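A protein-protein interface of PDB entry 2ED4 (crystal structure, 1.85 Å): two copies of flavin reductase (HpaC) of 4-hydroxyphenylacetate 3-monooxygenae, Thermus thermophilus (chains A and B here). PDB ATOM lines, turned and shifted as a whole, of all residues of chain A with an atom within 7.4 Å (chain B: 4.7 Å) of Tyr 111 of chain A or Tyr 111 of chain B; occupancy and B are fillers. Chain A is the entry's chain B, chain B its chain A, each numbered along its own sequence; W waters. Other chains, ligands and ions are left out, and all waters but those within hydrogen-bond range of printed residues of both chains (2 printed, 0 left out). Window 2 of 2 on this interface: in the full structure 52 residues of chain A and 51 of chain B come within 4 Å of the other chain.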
ATOM      1  N   LEU A  38      17.125  -7.172  20.122  1.00  0.00           N
ATOM      2  CA  LEU A  38      17.031  -8.393  19.336  1.00  0.00           C
ATOM      3  C   LEU A  38      16.063  -8.298  18.166  1.00  0.00           C
ATOM      4  O   LEU A  38      16.422  -8.600  17.029  1.00  0.00           O
ATOM      5  CB  LEU A  38      16.630  -9.564  20.238  1.00  0.00           C
ATOM      6  CG  LEU A  38      16.477 -10.932  19.569  1.00  0.00           C
ATOM      7  CD1 LEU A  38      17.779 -11.326  18.880  1.00  0.00           C
ATOM      8  CD2 LEU A  38      16.086 -11.960  20.621  1.00  0.00           C
ATOM      9  N   LEU A  47      19.640 -11.220  26.594  1.00  0.00           N
ATOM     10  CA  LEU A  47      20.646 -11.064  27.639  1.00  0.00           C
ATOM     11  C   LEU A  47      21.274 -12.419  27.948  1.00  0.00           C
ATOM     12  O   LEU A  47      20.688 -13.472  27.674  1.00  0.00           O
ATOM     13  CB  LEU A  47      20.031 -10.530  28.934  1.00  0.00           C
ATOM     14  CG  LEU A  47      19.294  -9.195  28.939  1.00  0.00           C
ATOM     15  CD1 LEU A  47      17.804  -9.435  29.087  1.00  0.00           C
ATOM     16  CD2 LEU A  47      19.810  -8.350  30.092  1.00  0.00           C
ATOM     17  N   GLU A  51      24.792 -19.217  34.492  1.00  0.00           N
ATOM     18  CA  GLU A  51      24.050 -20.362  35.003  1.00  0.00           C
ATOM     19  C   GLU A  51      24.232 -20.423  36.522  1.00  0.00           C
ATOM     20  O   GLU A  51      23.475 -21.101  37.226  1.00  0.00           O
ATOM     21  CB  GLU A  51      24.558 -21.647  34.347  1.00  0.00           C
ATOM     22  CG  GLU A  51      24.176 -21.785  32.877  1.00  0.00           C
ATOM     23  CD  GLU A  51      22.703 -22.123  32.666  1.00  0.00           C
ATOM     24  OE1 GLU A  51      22.007 -22.444  33.653  1.00  0.00           O
ATOM     25  OE2 GLU A  51      22.240 -22.075  31.505  1.00  0.00           O
ATOM     26  N   HIS A 108      10.068 -14.375  27.183  1.00  0.00           N
ATOM     27  CA  HIS A 108       9.658 -14.912  25.892  1.00  0.00           C
ATOM     28  C   HIS A 108      10.248 -16.283  25.573  1.00  0.00           C
ATOM     29  O   HIS A 108       9.561 -17.158  25.039  1.00  0.00           O
ATOM     30  CB  HIS A 108      10.036 -13.916  24.793  1.00  0.00           C
ATOM     31  CG  HIS A 108       9.490 -14.264  23.447  1.00  0.00           C
ATOM     32  ND1 HIS A 108       8.140 -14.257  23.168  1.00  0.00           N
ATOM     33  CD2 HIS A 108      10.110 -14.629  22.300  1.00  0.00           C
ATOM     34  CE1 HIS A 108       7.953 -14.605  21.907  1.00  0.00           C
ATOM     35  NE2 HIS A 108       9.131 -14.835  21.357  1.00  0.00           N
ATOM     36  N   ALA A 109      11.526 -16.467  25.894  1.00  0.00           N
ATOM     37  CA  ALA A 109      12.197 -17.734  25.638  1.00  0.00           C
ATOM     38  C   ALA A 109      13.571 -17.784  26.300  1.00  0.00           C
ATOM     39  O   ALA A 109      14.163 -16.748  26.621  1.00  0.00           O
ATOM     40  CB  ALA A 109      12.339 -17.958  24.130  1.00  0.00           C
ATOM     41  N   LEU A 110      14.063 -19.001  26.504  1.00  0.00           N
ATOM     42  CA  LEU A 110      15.372 -19.235  27.102  1.00  0.00           C
ATOM     43  C   LEU A 110      16.084 -20.261  26.227  1.00  0.00           C
ATOM     44  O   LEU A 110      15.448 -21.178  25.700  1.00  0.00           O
ATOM     45  CB  LEU A 110      15.229 -19.796  28.522  1.00  0.00           C
ATOM     46  CG  LEU A 110      14.568 -18.928  29.597  1.00  0.00           C
ATOM     47  CD1 LEU A 110      14.404 -19.742  30.877  1.00  0.00           C
ATOM     48  CD2 LEU A 110      15.419 -17.693  29.857  1.00  0.00           C
ATOM     49  N   TYR A 111      17.398 -20.104  26.070  1.00  0.00           N
ATOM     50  CA  TYR A 111      18.187 -21.024  25.257  1.00  0.00           C
ATOM     51  C   TYR A 111      19.516 -21.322  25.938  1.00  0.00           C
ATOM     52  O   TYR A 111      20.034 -20.504  26.705  1.00  0.00           O
ATOM     53  CB  TYR A 111      18.478 -20.417  23.882  1.00  0.00           C
ATOM     54  CG  TYR A 111      17.254 -20.019  23.093  1.00  0.00           C
ATOM     55  CD1 TYR A 111      16.417 -20.983  22.531  1.00  0.00           C
ATOM     56  CD2 TYR A 111      16.927 -18.675  22.915  1.00  0.00           C
ATOM     57  CE1 TYR A 111      15.276 -20.615  21.809  1.00  0.00           C
ATOM     58  CE2 TYR A 111      15.796 -18.297  22.197  1.00  0.00           C
ATOM     59  CZ  TYR A 111      14.974 -19.268  21.649  1.00  0.00           C
ATOM     60  OH  TYR A 111      13.848 -18.884  20.958  1.00  0.00           O
ATOM     61  N   PRO A 112      20.086 -22.507  25.670  1.00  0.00           N
ATOM     62  CA  PRO A 112      21.370 -22.869  26.273  1.00  0.00           C
ATOM     63  C   PRO A 112      22.413 -21.887  25.757  1.00  0.00           C
ATOM     64  O   PRO A 112      22.329 -21.438  24.614  1.00  0.00           O
ATOM     65  CB  PRO A 112      21.615 -24.280  25.743  1.00  0.00           C
ATOM     66  CG  PRO A 112      20.230 -24.817  25.539  1.00  0.00           C
ATOM     67  CD  PRO A 112      19.525 -23.638  24.909  1.00  0.00           C
ATOM     68  N   GLY A 113      23.394 -21.553  26.590  1.00  0.00           N
ATOM     69  CA  GLY A 113      24.426 -20.620  26.168  1.00  0.00           C
ATOM     70  C   GLY A 113      25.774 -20.888  26.814  1.00  0.00           C
ATOM     71  O   GLY A 113      26.453 -19.961  27.272  1.00  0.00           O
ATOM     72  N   GLY A 114      26.177 -22.156  26.845  1.00  0.00           N
ATOM     73  CA  GLY A 114      27.449 -22.503  27.457  1.00  0.00           C
ATOM     74  C   GLY A 114      27.330 -22.363  28.963  1.00  0.00           C
ATOM     75  O   GLY A 114      26.472 -23.006  29.574  1.00  0.00           O
ATOM     76  N   HIS A 116      26.366 -19.739  30.388  1.00  0.00           N
ATOM     77  CA  HIS A 116      25.335 -18.715  30.582  1.00  0.00           C
ATOM     78  C   HIS A 116      24.049 -19.198  29.914  1.00  0.00           C
ATOM     79  O   HIS A 116      24.070 -20.128  29.105  1.00  0.00           O
ATOM     80  CB  HIS A 116      25.720 -17.386  29.919  1.00  0.00           C
ATOM     81  CG  HIS A 116      26.666 -16.547  30.718  1.00  0.00           C
ATOM     82  ND1 HIS A 116      27.917 -16.986  31.096  1.00  0.00           N
ATOM     83  CD2 HIS A 116      26.568 -15.268  31.159  1.00  0.00           C
ATOM     84  CE1 HIS A 116      28.549 -16.015  31.734  1.00  0.00           C
ATOM     85  NE2 HIS A 116      27.753 -14.961  31.784  1.00  0.00           N
ATOM     86  N   ARG A 117      22.936 -18.558  30.250  1.00  0.00           N
ATOM     87  CA  ARG A 117      21.646 -18.894  29.653  1.00  0.00           C
ATOM     88  C   ARG A 117      21.236 -17.687  28.824  1.00  0.00           C
ATOM     89  O   ARG A 117      21.346 -16.552  29.286  1.00  0.00           O
ATOM     90  CB  ARG A 117      20.580 -19.123  30.727  1.00  0.00           C
ATOM     91  CG  ARG A 117      19.229 -19.613  30.179  1.00  0.00           C
ATOM     92  CD  ARG A 117      19.274 -21.123  29.894  1.00  0.00           C
ATOM     93  NE  ARG A 117      19.556 -21.864  31.120  1.00  0.00           N
ATOM     94  CZ  ARG A 117      18.660 -22.118  32.068  1.00  0.00           C
ATOM     95  NH1 ARG A 117      17.403 -21.708  31.936  1.00  0.00           N
ATOM     96  NH2 ARG A 117      19.030 -22.750  33.173  1.00  0.00           N
ATOM     97  N   ILE A 118      20.785 -17.918  27.598  1.00  0.00           N
ATOM     98  CA  ILE A 118      20.334 -16.813  26.770  1.00  0.00           C
ATOM     99  C   ILE A 118      18.893 -16.532  27.178  1.00  0.00           C
ATOM    100  O   ILE A 118      18.031 -17.407  27.088  1.00  0.00           O
ATOM    101  CB  ILE A 118      20.377 -17.160  25.272  1.00  0.00           C
ATOM    102  CG1 ILE A 118      21.826 -17.394  24.835  1.00  0.00           C
ATOM    103  CG2 ILE A 118      19.758 -16.025  24.465  1.00  0.00           C
ATOM    104  CD1 ILE A 118      21.977 -17.814  23.376  1.00  0.00           C
ATOM    105  N   VAL A 119      18.647 -15.313  27.642  1.00  0.00           N
ATOM    106  CA  VAL A 119      17.318 -14.904  28.079  1.00  0.00           C
ATOM    107  C   VAL A 119      16.722 -13.917  27.084  1.00  0.00           C
ATOM    108  O   VAL A 119      17.320 -12.876  26.797  1.00  0.00           O
ATOM    109  CB  VAL A 119      17.385 -14.223  29.473  1.00  0.00           C
ATOM    110  CG1 VAL A 119      16.006 -13.735  29.895  1.00  0.00           C
ATOM    111  CG2 VAL A 119      17.943 -15.199  30.497  1.00  0.00           C
ATOM    112  N   VAL A 120      15.545 -14.247  26.554  1.00  0.00           N
ATOM    113  CA  VAL A 120      14.865 -13.379  25.599  1.00  0.00           C
ATOM    114  C   VAL A 120      13.612 -12.789  26.237  1.00  0.00           C
ATOM    115  O   VAL A 120      12.765 -13.515  26.767  1.00  0.00           O
ATOM    116  CB  VAL A 120      14.458 -14.147  24.320  1.00  0.00           C
ATOM    117  CG1 VAL A 120      13.777 -13.203  23.345  1.00  0.00           C
ATOM    118  CG2 VAL A 120      15.692 -14.773  23.673  1.00  0.00           C
ATOM    119  N   ALA B 109      25.330 -22.440  17.262  1.00  0.00           N
ATOM    120  CA  ALA B 109      23.886 -22.611  17.301  1.00  0.00           C
ATOM    121  C   ALA B 109      23.165 -21.420  16.692  1.00  0.00           C
ATOM    122  O   ALA B 109      23.732 -20.334  16.561  1.00  0.00           O
ATOM    123  CB  ALA B 109      23.423 -22.807  18.739  1.00  0.00           C
ATOM    124  N   LEU B 110      21.911 -21.650  16.319  1.00  0.00           N
ATOM    125  CA  LEU B 110      21.046 -20.627  15.746  1.00  0.00           C
ATOM    126  C   LEU B 110      19.722 -20.771  16.482  1.00  0.00           C
ATOM    127  O   LEU B 110      19.144 -21.859  16.521  1.00  0.00           O
ATOM    128  CB  LEU B 110      20.830 -20.870  14.250  1.00  0.00           C
ATOM    129  CG  LEU B 110      22.072 -20.838  13.357  1.00  0.00           C
ATOM    130  CD1 LEU B 110      21.717 -21.337  11.962  1.00  0.00           C
ATOM    131  CD2 LEU B 110      22.628 -19.425  13.304  1.00  0.00           C
ATOM    132  N   TYR B 111      19.254 -19.684  17.081  1.00  0.00           N
ATOM    133  CA  TYR B 111      17.999 -19.712  17.822  1.00  0.00           C
ATOM    134  C   TYR B 111      17.067 -18.615  17.326  1.00  0.00           C
ATOM    135  O   TYR B 111      17.521 -17.565  16.865  1.00  0.00           O
ATOM    136  CB  TYR B 111      18.259 -19.504  19.316  1.00  0.00           C
ATOM    137  CG  TYR B 111      19.172 -20.530  19.956  1.00  0.00           C
ATOM    138  CD1 TYR B 111      18.834 -21.886  19.970  1.00  0.00           C
ATOM    139  CD2 TYR B 111      20.354 -20.140  20.586  1.00  0.00           C
ATOM    140  CE1 TYR B 111      19.653 -22.829  20.601  1.00  0.00           C
ATOM    141  CE2 TYR B 111      21.177 -21.070  21.219  1.00  0.00           C
ATOM    142  CZ  TYR B 111      20.822 -22.410  21.226  1.00  0.00           C
ATOM    143  OH  TYR B 111      21.622 -23.324  21.878  1.00  0.00           O
ATOM    144  N   PRO B 112      15.747 -18.844  17.422  1.00  0.00           N
ATOM    145  CA  PRO B 112      14.730 -17.879  16.990  1.00  0.00           C
ATOM    146  C   PRO B 112      14.863 -16.565  17.754  1.00  0.00           C
ATOM    147  O   PRO B 112      15.066 -16.569  18.969  1.00  0.00           O
ATOM    148  CB  PRO B 112      13.416 -18.585  17.321  1.00  0.00           C
ATOM    149  CG  PRO B 112      13.770 -20.042  17.207  1.00  0.00           C
ATOM    150  CD  PRO B 112      15.116 -20.090  17.894  1.00  0.00           C
ATOM    151  N   GLY B 113      14.745 -15.449  17.042  1.00  0.00           N
ATOM    152  CA  GLY B 113      14.847 -14.151  17.687  1.00  0.00           C
ATOM    153  C   GLY B 113      13.935 -13.115  17.059  1.00  0.00           C
ATOM    154  O   GLY B 113      14.358 -11.993  16.774  1.00  0.00           O
ATOM    155  N   ARG B 117      17.789 -13.470  13.919  1.00  0.00           N
ATOM    156  CA  ARG B 117      18.166 -14.812  14.331  1.00  0.00           C
ATOM    157  C   ARG B 117      19.290 -14.633  15.339  1.00  0.00           C
ATOM    158  O   ARG B 117      20.155 -13.778  15.158  1.00  0.00           O
ATOM    159  CB  ARG B 117      18.689 -15.623  13.143  1.00  0.00           C
ATOM    160  CG  ARG B 117      18.951 -17.093  13.456  1.00  0.00           C
ATOM    161  CD  ARG B 117      17.645 -17.862  13.584  1.00  0.00           C
ATOM    162  NE  ARG B 117      16.936 -17.910  12.307  1.00  0.00           N
ATOM    163  CZ  ARG B 117      17.223 -18.759  11.323  1.00  0.00           C
ATOM    164  NH1 ARG B 117      18.199 -19.644  11.465  1.00  0.00           N
ATOM    165  NH2 ARG B 117      16.547 -18.706  10.183  1.00  0.00           N
ATOM    166  N   ILE B 118      19.265 -15.418  16.408  1.00  0.00           N
ATOM    167  CA  ILE B 118      20.324 -15.351  17.405  1.00  0.00           C
ATOM    168  C   ILE B 118      21.454 -16.249  16.910  1.00  0.00           C
ATOM    169  O   ILE B 118      21.295 -17.468  16.812  1.00  0.00           O
ATOM    170  CB  ILE B 118      19.838 -15.848  18.777  1.00  0.00           C
ATOM    171  CG1 ILE B 118      18.764 -14.898  19.319  1.00  0.00           C
ATOM    172  CG2 ILE B 118      21.015 -15.946  19.745  1.00  0.00           C
ATOM    173  CD1 ILE B 118      18.172 -15.337  20.650  1.00  0.00           C
ATOM    174  N   VAL B 120      25.060 -17.824  17.514  1.00  0.00           N
ATOM    175  CA  VAL B 120      26.020 -18.141  18.565  1.00  0.00           C
ATOM    176  C   VAL B 120      27.305 -18.712  17.971  1.00  0.00           C
ATOM    177  O   VAL B 120      27.282 -19.718  17.260  1.00  0.00           O
ATOM    178  CB  VAL B 120      25.428 -19.163  19.564  1.00  0.00           C
ATOM    179  CG1 VAL B 120      26.433 -19.455  20.671  1.00  0.00           C
ATOM    180  CG2 VAL B 120      24.123 -18.626  20.150  1.00  0.00           C
HETATM  181  O   HOH W   1      13.271 -16.112  20.857  1.00  0.00           O
HETATM  182  O   HOH W   2      23.901 -22.358  22.721  1.00  0.00           O
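The backbone carbonyl oxygen (O) of Pro 112 of chain A is in hydrogen-bond range of the side-chain hydroxyl (OH) of Tyr 111 of chain B, 3.4 Å away.
OH of Tyr 111 of chain A is in hydrogen-bond range of O of Pro 112 of chain B, at 3.3 Å.
Tyr 111 of chain A touches its own counterpart, Tyr 111 of chain B.
Tyr 111 of chain A touches Pro 112 of chain B, and with the chains exchanged Pro 112 of chain A touches Tyr 111 of chain B.
Ile 118 of chain A touches Tyr 111 of chain B, but with the chains exchanged Tyr 111 of chain A does not touch Ile 118 of chain B (4.1 Å).
Ile 118 of chain A touches Val 120 of chain B, and with the chains exchanged Val 120 of chain A touches Ile 118 of chain B.
8 positions are printed for both chains.
CG of Leu 38 of chain A touches O of Gly 113 of chain B, 3.7 Å away.
Ile 118 of chain B touches Leu 38 of chain A (CG1 to CD1, 3.7 Å).
Tyr 111 of chain A touches Tyr 111 of chain B.
Tyr 111 of chain B touches Ile 118 of chain A.
CD1 of Ile 118 of chain A touches CG2 of Val 120 of chain B (3.96 Å).
Val 120 of chain A touches Ile 118 of chain B.
Water W2 bridges OH of Tyr 111 of chain B and O of Pro 112 of chain A.
Water W1 bridges the backbone carbonyl oxygen (O) of Pro 112 of chain B (2.6 Å) and the side-chain hydroxyl (OH) of Tyr 111 of chain A (2.8 Å).
The backbone NH of His 108 of chain A sits at hydrogen-bond distance from the backbone carbonyl oxygen of Val 120 of chain A, at 2.9 Å.
O of Tyr 111 of chain B sits at hydrogen-bond distance from N of Ile 118 of chain B, at 2.8 Å.
O of Tyr 111 of chain A sits at hydrogen-bond distance from N of Ile 118 of chain A, 2.8 Å away.
O of Ala 109 of chain A lies within hydrogen-bond range of N of Val 120 of chain A (2.9 Å).
The backbone carbonyl oxygen (O) of Ala 109 of chain B lies within hydrogen-bond range of the backbone NH (N) of Val 120 of chain B, 3.0 Å away.
Of the 15 printed residues of chain A, 5 touch a printed residue of chain B.
Printed residues of chain A that touch a printed residue of chain B: Leu 38, Tyr 111, Pro 112, Ile 118 and Val 120.
Hydrophobic or aromatic side chains of chain A within 4 Å of the printed part of chain B: Leu 38, Tyr 111, Pro 112, Ile 118 and Val 120.
Of the 8 printed residues of chain B, 5 touch a printed residue of chain A.
Printed residues of chain B that touch a printed residue of chain A: Tyr 111, Pro 112, Gly 113, Ile 118 and Val 120.
Among the printed residues, 8 pairs touch across the chains.
Among the printed residues, no Asp or Glu carboxylate lies within 4 Å of a Lys or Arg side-chain nitrogen of the other chain.
Of chain B, only Tyr 111 and Pro 112 come within 4 Å of Tyr 111 of chain A.
Of the printed residues of chain B, Pro 112 of chain A touches Tyr 111 (3.4 Å).
Of the printed residues of chain B, Ile 118 of chain A touches Tyr 111 and Val 120.
Of the printed residues of chain A, Gly 113 of chain B touches Leu 38.
Of the printed residues of chain A, Val 120 of chain B touches Ile 118 (3.96 Å).
The nearest residue of chain A that does not touch Tyr 111 of chain B is Gly 113 of chain A (5.3 Å).
The nearest printed residue of chain A that does not touch Val 120 of chain B is Pro 112 of chain A (5.6 Å).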
